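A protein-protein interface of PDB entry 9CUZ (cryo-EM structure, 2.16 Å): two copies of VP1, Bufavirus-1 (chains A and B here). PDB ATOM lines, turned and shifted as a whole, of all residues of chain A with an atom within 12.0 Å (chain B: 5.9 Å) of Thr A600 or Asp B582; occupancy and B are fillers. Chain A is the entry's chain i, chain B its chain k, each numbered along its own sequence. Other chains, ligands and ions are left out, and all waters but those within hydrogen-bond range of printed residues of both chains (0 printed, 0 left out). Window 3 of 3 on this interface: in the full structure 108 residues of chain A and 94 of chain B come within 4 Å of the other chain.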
ATOM      1  N   THR A 596      21.105 -16.647  18.404  1.00  0.00           N
ATOM      2  CA  THR A 596      20.015 -16.329  17.496  1.00  0.00           C
ATOM      3  C   THR A 596      20.478 -15.277  16.492  1.00  0.00           C
ATOM      4  O   THR A 596      20.980 -14.229  16.897  1.00  0.00           O
ATOM      5  CB  THR A 596      18.822 -15.785  18.271  1.00  0.00           C
ATOM      6  OG1 THR A 596      18.420 -16.729  19.259  1.00  0.00           O
ATOM      7  CG2 THR A 596      17.681 -15.558  17.340  1.00  0.00           C
ATOM      8  N   PRO A 597      20.317 -15.507  15.195  1.00  0.00           N
ATOM      9  CA  PRO A 597      20.643 -14.455  14.228  1.00  0.00           C
ATOM     10  C   PRO A 597      19.749 -13.247  14.427  1.00  0.00           C
ATOM     11  O   PRO A 597      18.558 -13.369  14.709  1.00  0.00           O
ATOM     12  CB  PRO A 597      20.390 -15.127  12.877  1.00  0.00           C
ATOM     13  CG  PRO A 597      19.401 -16.170  13.170  1.00  0.00           C
ATOM     14  CD  PRO A 597      19.743 -16.689  14.534  1.00  0.00           C
ATOM     15  N   ASP A 598      20.330 -12.060  14.289  1.00  0.00           N
ATOM     16  CA  ASP A 598      19.517 -10.866  14.462  1.00  0.00           C
ATOM     17  C   ASP A 598      18.992 -10.446  13.093  1.00  0.00           C
ATOM     18  O   ASP A 598      19.676  -9.854  12.266  1.00  0.00           O
ATOM     19  CB  ASP A 598      20.339  -9.763  15.121  1.00  0.00           C
ATOM     20  CG  ASP A 598      19.502  -8.564  15.536  1.00  0.00           C
ATOM     21  OD1 ASP A 598      18.262  -8.620  15.424  1.00  0.00           O
ATOM     22  OD2 ASP A 598      20.090  -7.551  15.956  1.00  0.00           O
ATOM     23  N   THR A 599      17.770 -10.919  12.813  1.00  0.00           N
ATOM     24  CA  THR A 599      17.090 -10.613  11.529  1.00  0.00           C
ATOM     25  C   THR A 599      15.634 -10.267  11.864  1.00  0.00           C
ATOM     26  O   THR A 599      15.252 -10.450  13.030  1.00  0.00           O
ATOM     27  CB  THR A 599      17.141 -11.806  10.567  1.00  0.00           C
ATOM     28  OG1 THR A 599      16.519 -12.927  11.193  1.00  0.00           O
ATOM     29  CG2 THR A 599      18.549 -12.169  10.147  1.00  0.00           C
ATOM     30  N   THR A 600      14.846  -9.823  10.885  1.00  0.00           N
ATOM     31  CA  THR A 600      13.409  -9.528  11.136  1.00  0.00           C
ATOM     32  C   THR A 600      12.677 -10.817  11.533  1.00  0.00           C
ATOM     33  O   THR A 600      11.976 -10.802  12.560  1.00  0.00           O
ATOM     34  CB  THR A 600      12.760  -8.852   9.919  1.00  0.00           C
ATOM     35  OG1 THR A 600      13.524  -7.690   9.594  1.00  0.00           O
ATOM     36  CG2 THR A 600      11.316  -8.471  10.159  1.00  0.00           C
ATOM     37  N   HIS A 601      12.842 -11.885  10.750  1.00  0.00           N
ATOM     38  CA  HIS A 601      12.154 -13.171  11.041  1.00  0.00           C
ATOM     39  C   HIS A 601      13.154 -14.137  11.680  1.00  0.00           C
ATOM     40  O   HIS A 601      14.083 -14.576  10.980  1.00  0.00           O
ATOM     41  CB  HIS A 601      11.507 -13.758   9.778  1.00  0.00           C
ATOM     42  CG  HIS A 601      10.928 -15.116   9.986  1.00  0.00           C
ATOM     43  ND1 HIS A 601      11.636 -16.271   9.715  1.00  0.00           N
ATOM     44  CD2 HIS A 601       9.720 -15.510  10.444  1.00  0.00           C
ATOM     45  CE1 HIS A 601      10.887 -17.318   9.993  1.00  0.00           C
ATOM     46  NE2 HIS A 601       9.707 -16.880  10.441  1.00  0.00           N
ATOM     47  N   LYS A 602      12.973 -14.428  12.967  1.00  0.00           N
ATOM     48  CA  LYS A 602      13.886 -15.356  13.679  1.00  0.00           C
ATOM     49  C   LYS A 602      13.580 -16.776  13.213  1.00  0.00           C
ATOM     50  O   LYS A 602      12.397 -17.068  12.968  1.00  0.00           O
ATOM     51  CB  LYS A 602      13.693 -15.247  15.194  1.00  0.00           C
ATOM     52  CG  LYS A 602      14.724 -14.392  15.918  1.00  0.00           C
ATOM     53  CD  LYS A 602      14.937 -13.032  15.293  1.00  0.00           C
ATOM     54  CE  LYS A 602      15.909 -12.179  16.081  1.00  0.00           C
ATOM     55  NZ  LYS A 602      16.175 -10.884  15.413  1.00  0.00           N
ATOM     56  N   PRO A 603      14.584 -17.658  13.045  1.00  0.00           N
ATOM     57  CA  PRO A 603      14.308 -19.051  12.684  1.00  0.00           C
ATOM     58  C   PRO A 603      13.429 -19.713  13.728  1.00  0.00           C
ATOM     59  O   PRO A 603      13.528 -19.430  14.919  1.00  0.00           O
ATOM     60  CB  PRO A 603      15.699 -19.689  12.643  1.00  0.00           C
ATOM     61  CG  PRO A 603      16.616 -18.572  12.404  1.00  0.00           C
ATOM     62  CD  PRO A 603      16.028 -17.399  13.131  1.00  0.00           C
ATOM     63  N   MET A 604      12.567 -20.601  13.267  1.00  0.00           N
ATOM     64  CA  MET A 604      11.645 -21.287  14.157  1.00  0.00           C
ATOM     65  C   MET A 604      12.323 -22.385  14.960  1.00  0.00           C
ATOM     66  O   MET A 604      11.880 -22.687  16.066  1.00  0.00           O
ATOM     67  CB  MET A 604      10.507 -21.880  13.335  1.00  0.00           C
ATOM     68  CG  MET A 604       9.748 -20.842  12.551  1.00  0.00           C
ATOM     69  SD  MET A 604       8.532 -21.570  11.454  1.00  0.00           S
ATOM     70  CE  MET A 604       8.064 -20.113  10.558  1.00  0.00           C
ATOM     71  N   LYS A 614      17.837 -17.089  23.630  1.00  0.00           N
ATOM     72  CA  LYS A 614      16.903 -16.050  23.205  1.00  0.00           C
ATOM     73  C   LYS A 614      17.561 -14.682  23.267  1.00  0.00           C
ATOM     74  O   LYS A 614      17.463 -13.884  22.333  1.00  0.00           O
ATOM     75  CB  LYS A 614      15.643 -16.085  24.065  1.00  0.00           C
ATOM     76  CG  LYS A 614      14.817 -17.333  23.878  1.00  0.00           C
ATOM     77  CD  LYS A 614      13.640 -17.367  24.835  1.00  0.00           C
ATOM     78  CE  LYS A 614      12.824 -18.624  24.653  1.00  0.00           C
ATOM     79  NZ  LYS A 614      11.703 -18.699  25.627  1.00  0.00           N
ATOM     80  N   THR B 413      11.576  -1.576  14.038  1.00  0.00           N
ATOM     81  CA  THR B 413      12.207  -1.908  12.769  1.00  0.00           C
ATOM     82  C   THR B 413      13.706  -1.693  12.875  1.00  0.00           C
ATOM     83  O   THR B 413      14.162  -0.764  13.541  1.00  0.00           O
ATOM     84  CB  THR B 413      11.649  -1.077  11.609  1.00  0.00           C
ATOM     85  OG1 THR B 413      11.852   0.318  11.860  1.00  0.00           O
ATOM     86  CG2 THR B 413      10.192  -1.331  11.457  1.00  0.00           C
ATOM     87  N   GLN B 414      14.463  -2.559  12.216  1.00  0.00           N
ATOM     88  CA  GLN B 414      15.913  -2.485  12.234  1.00  0.00           C
ATOM     89  C   GLN B 414      16.400  -1.407  11.281  1.00  0.00           C
ATOM     90  O   GLN B 414      15.928  -1.291  10.153  1.00  0.00           O
ATOM     91  CB  GLN B 414      16.524  -3.828  11.843  1.00  0.00           C
ATOM     92  CG  GLN B 414      16.289  -4.947  12.824  1.00  0.00           C
ATOM     93  CD  GLN B 414      16.828  -6.275  12.320  1.00  0.00           C
ATOM     94  OE1 GLN B 414      16.943  -6.492  11.117  1.00  0.00           O
ATOM     95  NE2 GLN B 414      17.156  -7.169  13.242  1.00  0.00           N
ATOM     96  N   HIS B 418      22.096  -6.213   6.701  1.00  0.00           N
ATOM     97  CA  HIS B 418      22.871  -7.399   7.030  1.00  0.00           C
ATOM     98  C   HIS B 418      23.570  -7.915   5.783  1.00  0.00           C
ATOM     99  O   HIS B 418      22.926  -8.162   4.762  1.00  0.00           O
ATOM    100  CB  HIS B 418      21.983  -8.462   7.666  1.00  0.00           C
ATOM    101  CG  HIS B 418      21.418  -8.045   8.986  1.00  0.00           C
ATOM    102  ND1 HIS B 418      20.073  -7.822   9.175  1.00  0.00           N
ATOM    103  CD2 HIS B 418      22.007  -7.808  10.178  1.00  0.00           C
ATOM    104  CE1 HIS B 418      19.858  -7.472  10.429  1.00  0.00           C
ATOM    105  NE2 HIS B 418      21.017  -7.451  11.058  1.00  0.00           N
ATOM    106  N   PRO B 493      13.069  -9.715   0.102  1.00  0.00           N
ATOM    107  CA  PRO B 493      13.950  -8.661  -0.412  1.00  0.00           C
ATOM    108  C   PRO B 493      15.419  -9.039  -0.307  1.00  0.00           C
ATOM    109  O   PRO B 493      15.878  -9.525   0.727  1.00  0.00           O
ATOM    110  CB  PRO B 493      13.622  -7.470   0.491  1.00  0.00           C
ATOM    111  CG  PRO B 493      13.219  -8.098   1.775  1.00  0.00           C
ATOM    112  CD  PRO B 493      12.535  -9.382   1.433  1.00  0.00           C
ATOM    113  N   ILE B 539      21.571  -5.039   0.811  1.00  0.00           N
ATOM    114  CA  ILE B 539      21.142  -6.216   1.547  1.00  0.00           C
ATOM    115  C   ILE B 539      21.663  -7.425   0.795  1.00  0.00           C
ATOM    116  O   ILE B 539      21.011  -7.940  -0.114  1.00  0.00           O
ATOM    117  CB  ILE B 539      19.604  -6.275   1.651  1.00  0.00           C
ATOM    118  CG1 ILE B 539      19.030  -5.124   2.468  1.00  0.00           C
ATOM    119  CG2 ILE B 539      19.134  -7.586   2.250  1.00  0.00           C
ATOM    120  CD1 ILE B 539      17.516  -5.066   2.394  1.00  0.00           C
ATOM    121  N   GLN B 542      21.352 -12.392   2.420  1.00  0.00           N
ATOM    122  CA  GLN B 542      20.125 -13.111   2.130  1.00  0.00           C
ATOM    123  C   GLN B 542      19.848 -13.167   0.638  1.00  0.00           C
ATOM    124  O   GLN B 542      18.765 -13.600   0.245  1.00  0.00           O
ATOM    125  CB  GLN B 542      18.912 -12.578   2.907  1.00  0.00           C
ATOM    126  CG  GLN B 542      18.293 -11.250   2.564  1.00  0.00           C
ATOM    127  CD  GLN B 542      17.102 -10.981   3.476  1.00  0.00           C
ATOM    128  OE1 GLN B 542      17.028 -11.512   4.572  1.00  0.00           O
ATOM    129  NE2 GLN B 542      16.142 -10.213   2.998  1.00  0.00           N
ATOM    130  N   VAL B 580      15.320 -14.350   7.930  1.00  0.00           N
ATOM    131  CA  VAL B 580      15.222 -13.406   6.784  1.00  0.00           C
ATOM    132  C   VAL B 580      14.752 -12.024   7.243  1.00  0.00           C
ATOM    133  O   VAL B 580      13.861 -11.956   8.098  1.00  0.00           O
ATOM    134  CB  VAL B 580      14.292 -13.985   5.699  1.00  0.00           C
ATOM    135  CG1 VAL B 580      12.914 -14.320   6.249  1.00  0.00           C
ATOM    136  CG2 VAL B 580      14.182 -13.066   4.492  1.00  0.00           C
ATOM    137  N   ASP B 581      15.295 -10.975   6.641  1.00  0.00           N
ATOM    138  CA  ASP B 581      14.976  -9.582   6.931  1.00  0.00           C
ATOM    139  C   ASP B 581      13.843  -9.064   6.055  1.00  0.00           C
ATOM    140  O   ASP B 581      13.699  -9.470   4.904  1.00  0.00           O
ATOM    141  CB  ASP B 581      16.179  -8.684   6.694  1.00  0.00           C
ATOM    142  CG  ASP B 581      17.210  -8.805   7.753  1.00  0.00           C
ATOM    143  OD1 ASP B 581      16.884  -9.265   8.856  1.00  0.00           O
ATOM    144  OD2 ASP B 581      18.362  -8.459   7.462  1.00  0.00           O
ATOM    145  N   ASP B 582      13.034  -8.162   6.609  1.00  0.00           N
ATOM    146  CA  ASP B 582      12.127  -7.407   5.756  1.00  0.00           C
ATOM    147  C   ASP B 582      12.852  -6.209   5.131  1.00  0.00           C
ATOM    148  O   ASP B 582      14.024  -5.950   5.403  1.00  0.00           O
ATOM    149  CB  ASP B 582      10.884  -6.961   6.533  1.00  0.00           C
ATOM    150  CG  ASP B 582      11.187  -5.986   7.670  1.00  0.00           C
ATOM    151  OD1 ASP B 582      12.360  -5.656   7.933  1.00  0.00           O
ATOM    152  OD2 ASP B 582      10.223  -5.551   8.325  1.00  0.00           O
ATOM    153  N   VAL B 583      12.161  -5.501   4.237  1.00  0.00           N
ATOM    154  CA  VAL B 583      12.826  -4.397   3.477  1.00  0.00           C
ATOM    155  C   VAL B 583      13.222  -3.227   4.390  1.00  0.00           C
ATOM    156  O   VAL B 583      14.296  -2.651   4.151  1.00  0.00           O
ATOM    157  CB  VAL B 583      11.941  -3.927   2.305  1.00  0.00           C
ATOM    158  CG1 VAL B 583      10.602  -3.387   2.787  1.00  0.00           C
ATOM    159  CG2 VAL B 583      12.652  -2.903   1.435  1.00  0.00           C
ATOM    160  N   GLY B 584      12.412  -2.891   5.397  1.00  0.00           N
ATOM    161  CA  GLY B 584      12.703  -1.736   6.216  1.00  0.00           C
ATOM    162  C   GLY B 584      12.179  -0.447   5.617  1.00  0.00           C
ATOM    163  O   GLY B 584      11.571  -0.410   4.546  1.00  0.00           O
ATOM    164  N   MET B 605       5.514 -11.249   8.554  1.00  0.00           N
ATOM    165  CA  MET B 605       6.268 -10.034   8.294  1.00  0.00           C
ATOM    166  C   MET B 605       5.658  -9.331   7.089  1.00  0.00           C
ATOM    167  O   MET B 605       4.850  -9.907   6.360  1.00  0.00           O
ATOM    168  CB  MET B 605       7.752 -10.385   8.152  1.00  0.00           C
ATOM    169  CG  MET B 605       8.077 -11.283   7.013  1.00  0.00           C
ATOM    170  SD  MET B 605       9.769 -11.902   7.162  1.00  0.00           S
ATOM    171  CE  MET B 605      10.737 -10.494   6.744  1.00  0.00           C
ATOM    172  N   SER B 606       5.997  -8.063   6.933  1.00  0.00           N
ATOM    173  CA  SER B 606       5.413  -7.221   5.902  1.00  0.00           C
ATOM    174  C   SER B 606       6.356  -7.074   4.716  1.00  0.00           C
ATOM    175  O   SER B 606       7.567  -6.941   4.875  1.00  0.00           O
ATOM    176  CB  SER B 606       5.071  -5.846   6.469  1.00  0.00           C
ATOM    177  OG  SER B 606       4.569  -5.011   5.456  1.00  0.00           O
ATOM    178  N   ALA B 609       5.422  -2.076   4.199  1.00  0.00           N
ATOM    179  CA  ALA B 609       5.316  -1.186   5.347  1.00  0.00           C
ATOM    180  C   ALA B 609       6.149  -1.709   6.515  1.00  0.00           C
ATOM    181  O   ALA B 609       6.038  -2.887   6.866  1.00  0.00           O
ATOM    182  CB  ALA B 609       3.861  -1.016   5.774  1.00  0.00           C
ATOM    183  N   PRO B 610       6.999  -0.885   7.122  1.00  0.00           N
ATOM    184  CA  PRO B 610       7.857  -1.401   8.194  1.00  0.00           C
ATOM    185  C   PRO B 610       7.111  -1.767   9.467  1.00  0.00           C
ATOM    186  O   PRO B 610       7.575  -2.651  10.189  1.00  0.00           O
ATOM    187  CB  PRO B 610       8.849  -0.253   8.415  1.00  0.00           C
ATOM    188  CG  PRO B 610       8.133   0.952   7.959  1.00  0.00           C
ATOM    189  CD  PRO B 610       7.310   0.515   6.796  1.00  0.00           C
ATOM    190  N   ARG B 700      17.688   0.987   5.991  1.00  0.00           N
ATOM    191  CA  ARG B 700      18.758   0.148   6.516  1.00  0.00           C
ATOM    192  C   ARG B 700      20.003   0.707   5.848  1.00  0.00           C
ATOM    193  O   ARG B 700      20.366   0.349   4.726  1.00  0.00           O
ATOM    194  CB  ARG B 700      18.535  -1.316   6.143  1.00  0.00           C
ATOM    195  CG  ARG B 700      17.316  -2.024   6.729  1.00  0.00           C
ATOM    196  CD  ARG B 700      17.275  -3.467   6.221  1.00  0.00           C
ATOM    197  NE  ARG B 700      16.180  -4.270   6.748  1.00  0.00           N
ATOM    198  CZ  ARG B 700      16.231  -4.939   7.896  1.00  0.00           C
ATOM    199  NH1 ARG B 700      17.327  -4.912   8.632  1.00  0.00           N
ATOM    200  NH2 ARG B 700      15.194  -5.648   8.298  1.00  0.00           N
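The side-chain amide nitrogen (NE2) of Gln B414 sits at hydrogen-bond distance from the side-chain carboxylate (OD1) of Asp A598.
A ring nitrogen (NE2) of His B418 sits at hydrogen-bond distance from the backbone carbonyl oxygen of Asp A598, at 3.0 Å.
The side-chain carboxylate of Asp B581 lies within hydrogen-bond range of the backbone NH of Thr A600 (2.9 Å).
The side-chain carboxylate of Asp B582 sits at hydrogen-bond distance from the side-chain hydroxyl of Thr A600, 2.9 Å away.
NH2 of Arg B700 sits at hydrogen-bond distance from OG1 of Thr A600 (2.9 Å).
N of His A601 is in hydrogen-bond range of O of Val B580 (2.8 Å).
The side-chain carboxylate (OD1) of Asp A598 lies within salt-bridge range of the side-chain amino group (NZ) of Lys A602 (3.1 Å).
O of His A601 is in hydrogen-bond range of OG1 of Thr A599 (2.9 Å).
The backbone carbonyl oxygen of Thr A599 lies within hydrogen-bond range of the side-chain amino group of Lys A602 (2.6 Å).
OD2 of Asp B581 sits at hydrogen-bond distance from ND1 of His B418.
The backbone NH (N) of Asp B581 lies within hydrogen-bond range of the side-chain amide oxygen (OE1) of Gln B542 (2.8 Å).
The side-chain carboxylate of Asp B582 lies within salt-bridge range of the guanidinium group of Arg B700 (2.9 Å).
Gln B414 touches Thr A599.
Val B580 touches Thr A599.
Asp B581 touches Thr A599.
Thr A600 touches Gln B414 (OG1 to OE1, 3.9 Å).
Thr A600 touches Val B580 (N to O, 3.6 Å).
Met B605 touches His A601 (SD to CB, 3.6 Å).
Asp B582 touches just one residue of chain A: Thr A600 (2.9 Å).
Thr B413 touches none of the printed residues of chain A.
Of the printed residues of chain A, Gln B414 touches Asp A598, Thr A599 and Thr A600.
Val B580 touches just these residues of chain A: Thr A599 (3.8 Å), Thr A600 (3.6 Å) and His A601 (2.8 Å).
No residue of chain A comes within 4 Å of Gly B584.
No residue of chain A comes within 4 Å of Ser B606.
No residue of chain A comes within 4 Å of Pro B610.
Of the printed residues of chain A, Arg B700 touches Thr A600.
Printed residues of chain B within 4 Å of Asp A598: Gln B414 (2.8 Å) and His B418 (3.0 Å).
Printed residues of chain A within 4 Å of His B418: Asp A598.
Ala B609 touches none of the printed residues of chain A.
The nearest printed residue of chain B that does not touch Thr A600 is Met B605 (4.01 Å).
The nearest printed residue of chain A that does not touch Met B605 is Thr A600 (4.01 Å).
Hydrophobic or aromatic side chains of chain A that line the printed part of chain B: His A601.
Hydrophobic or aromatic side chains of chain B within 4 Å of the printed part of chain A: His B418, Val B580 and Met B605.
Among the printed residues, 12 pairs touch across the chains.
Among the printed residues, no Asp or Glu carboxylate lies within 4 Å of a Lys or Arg side-chain nitrogen of the other chain.
No position is printed for both chains.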
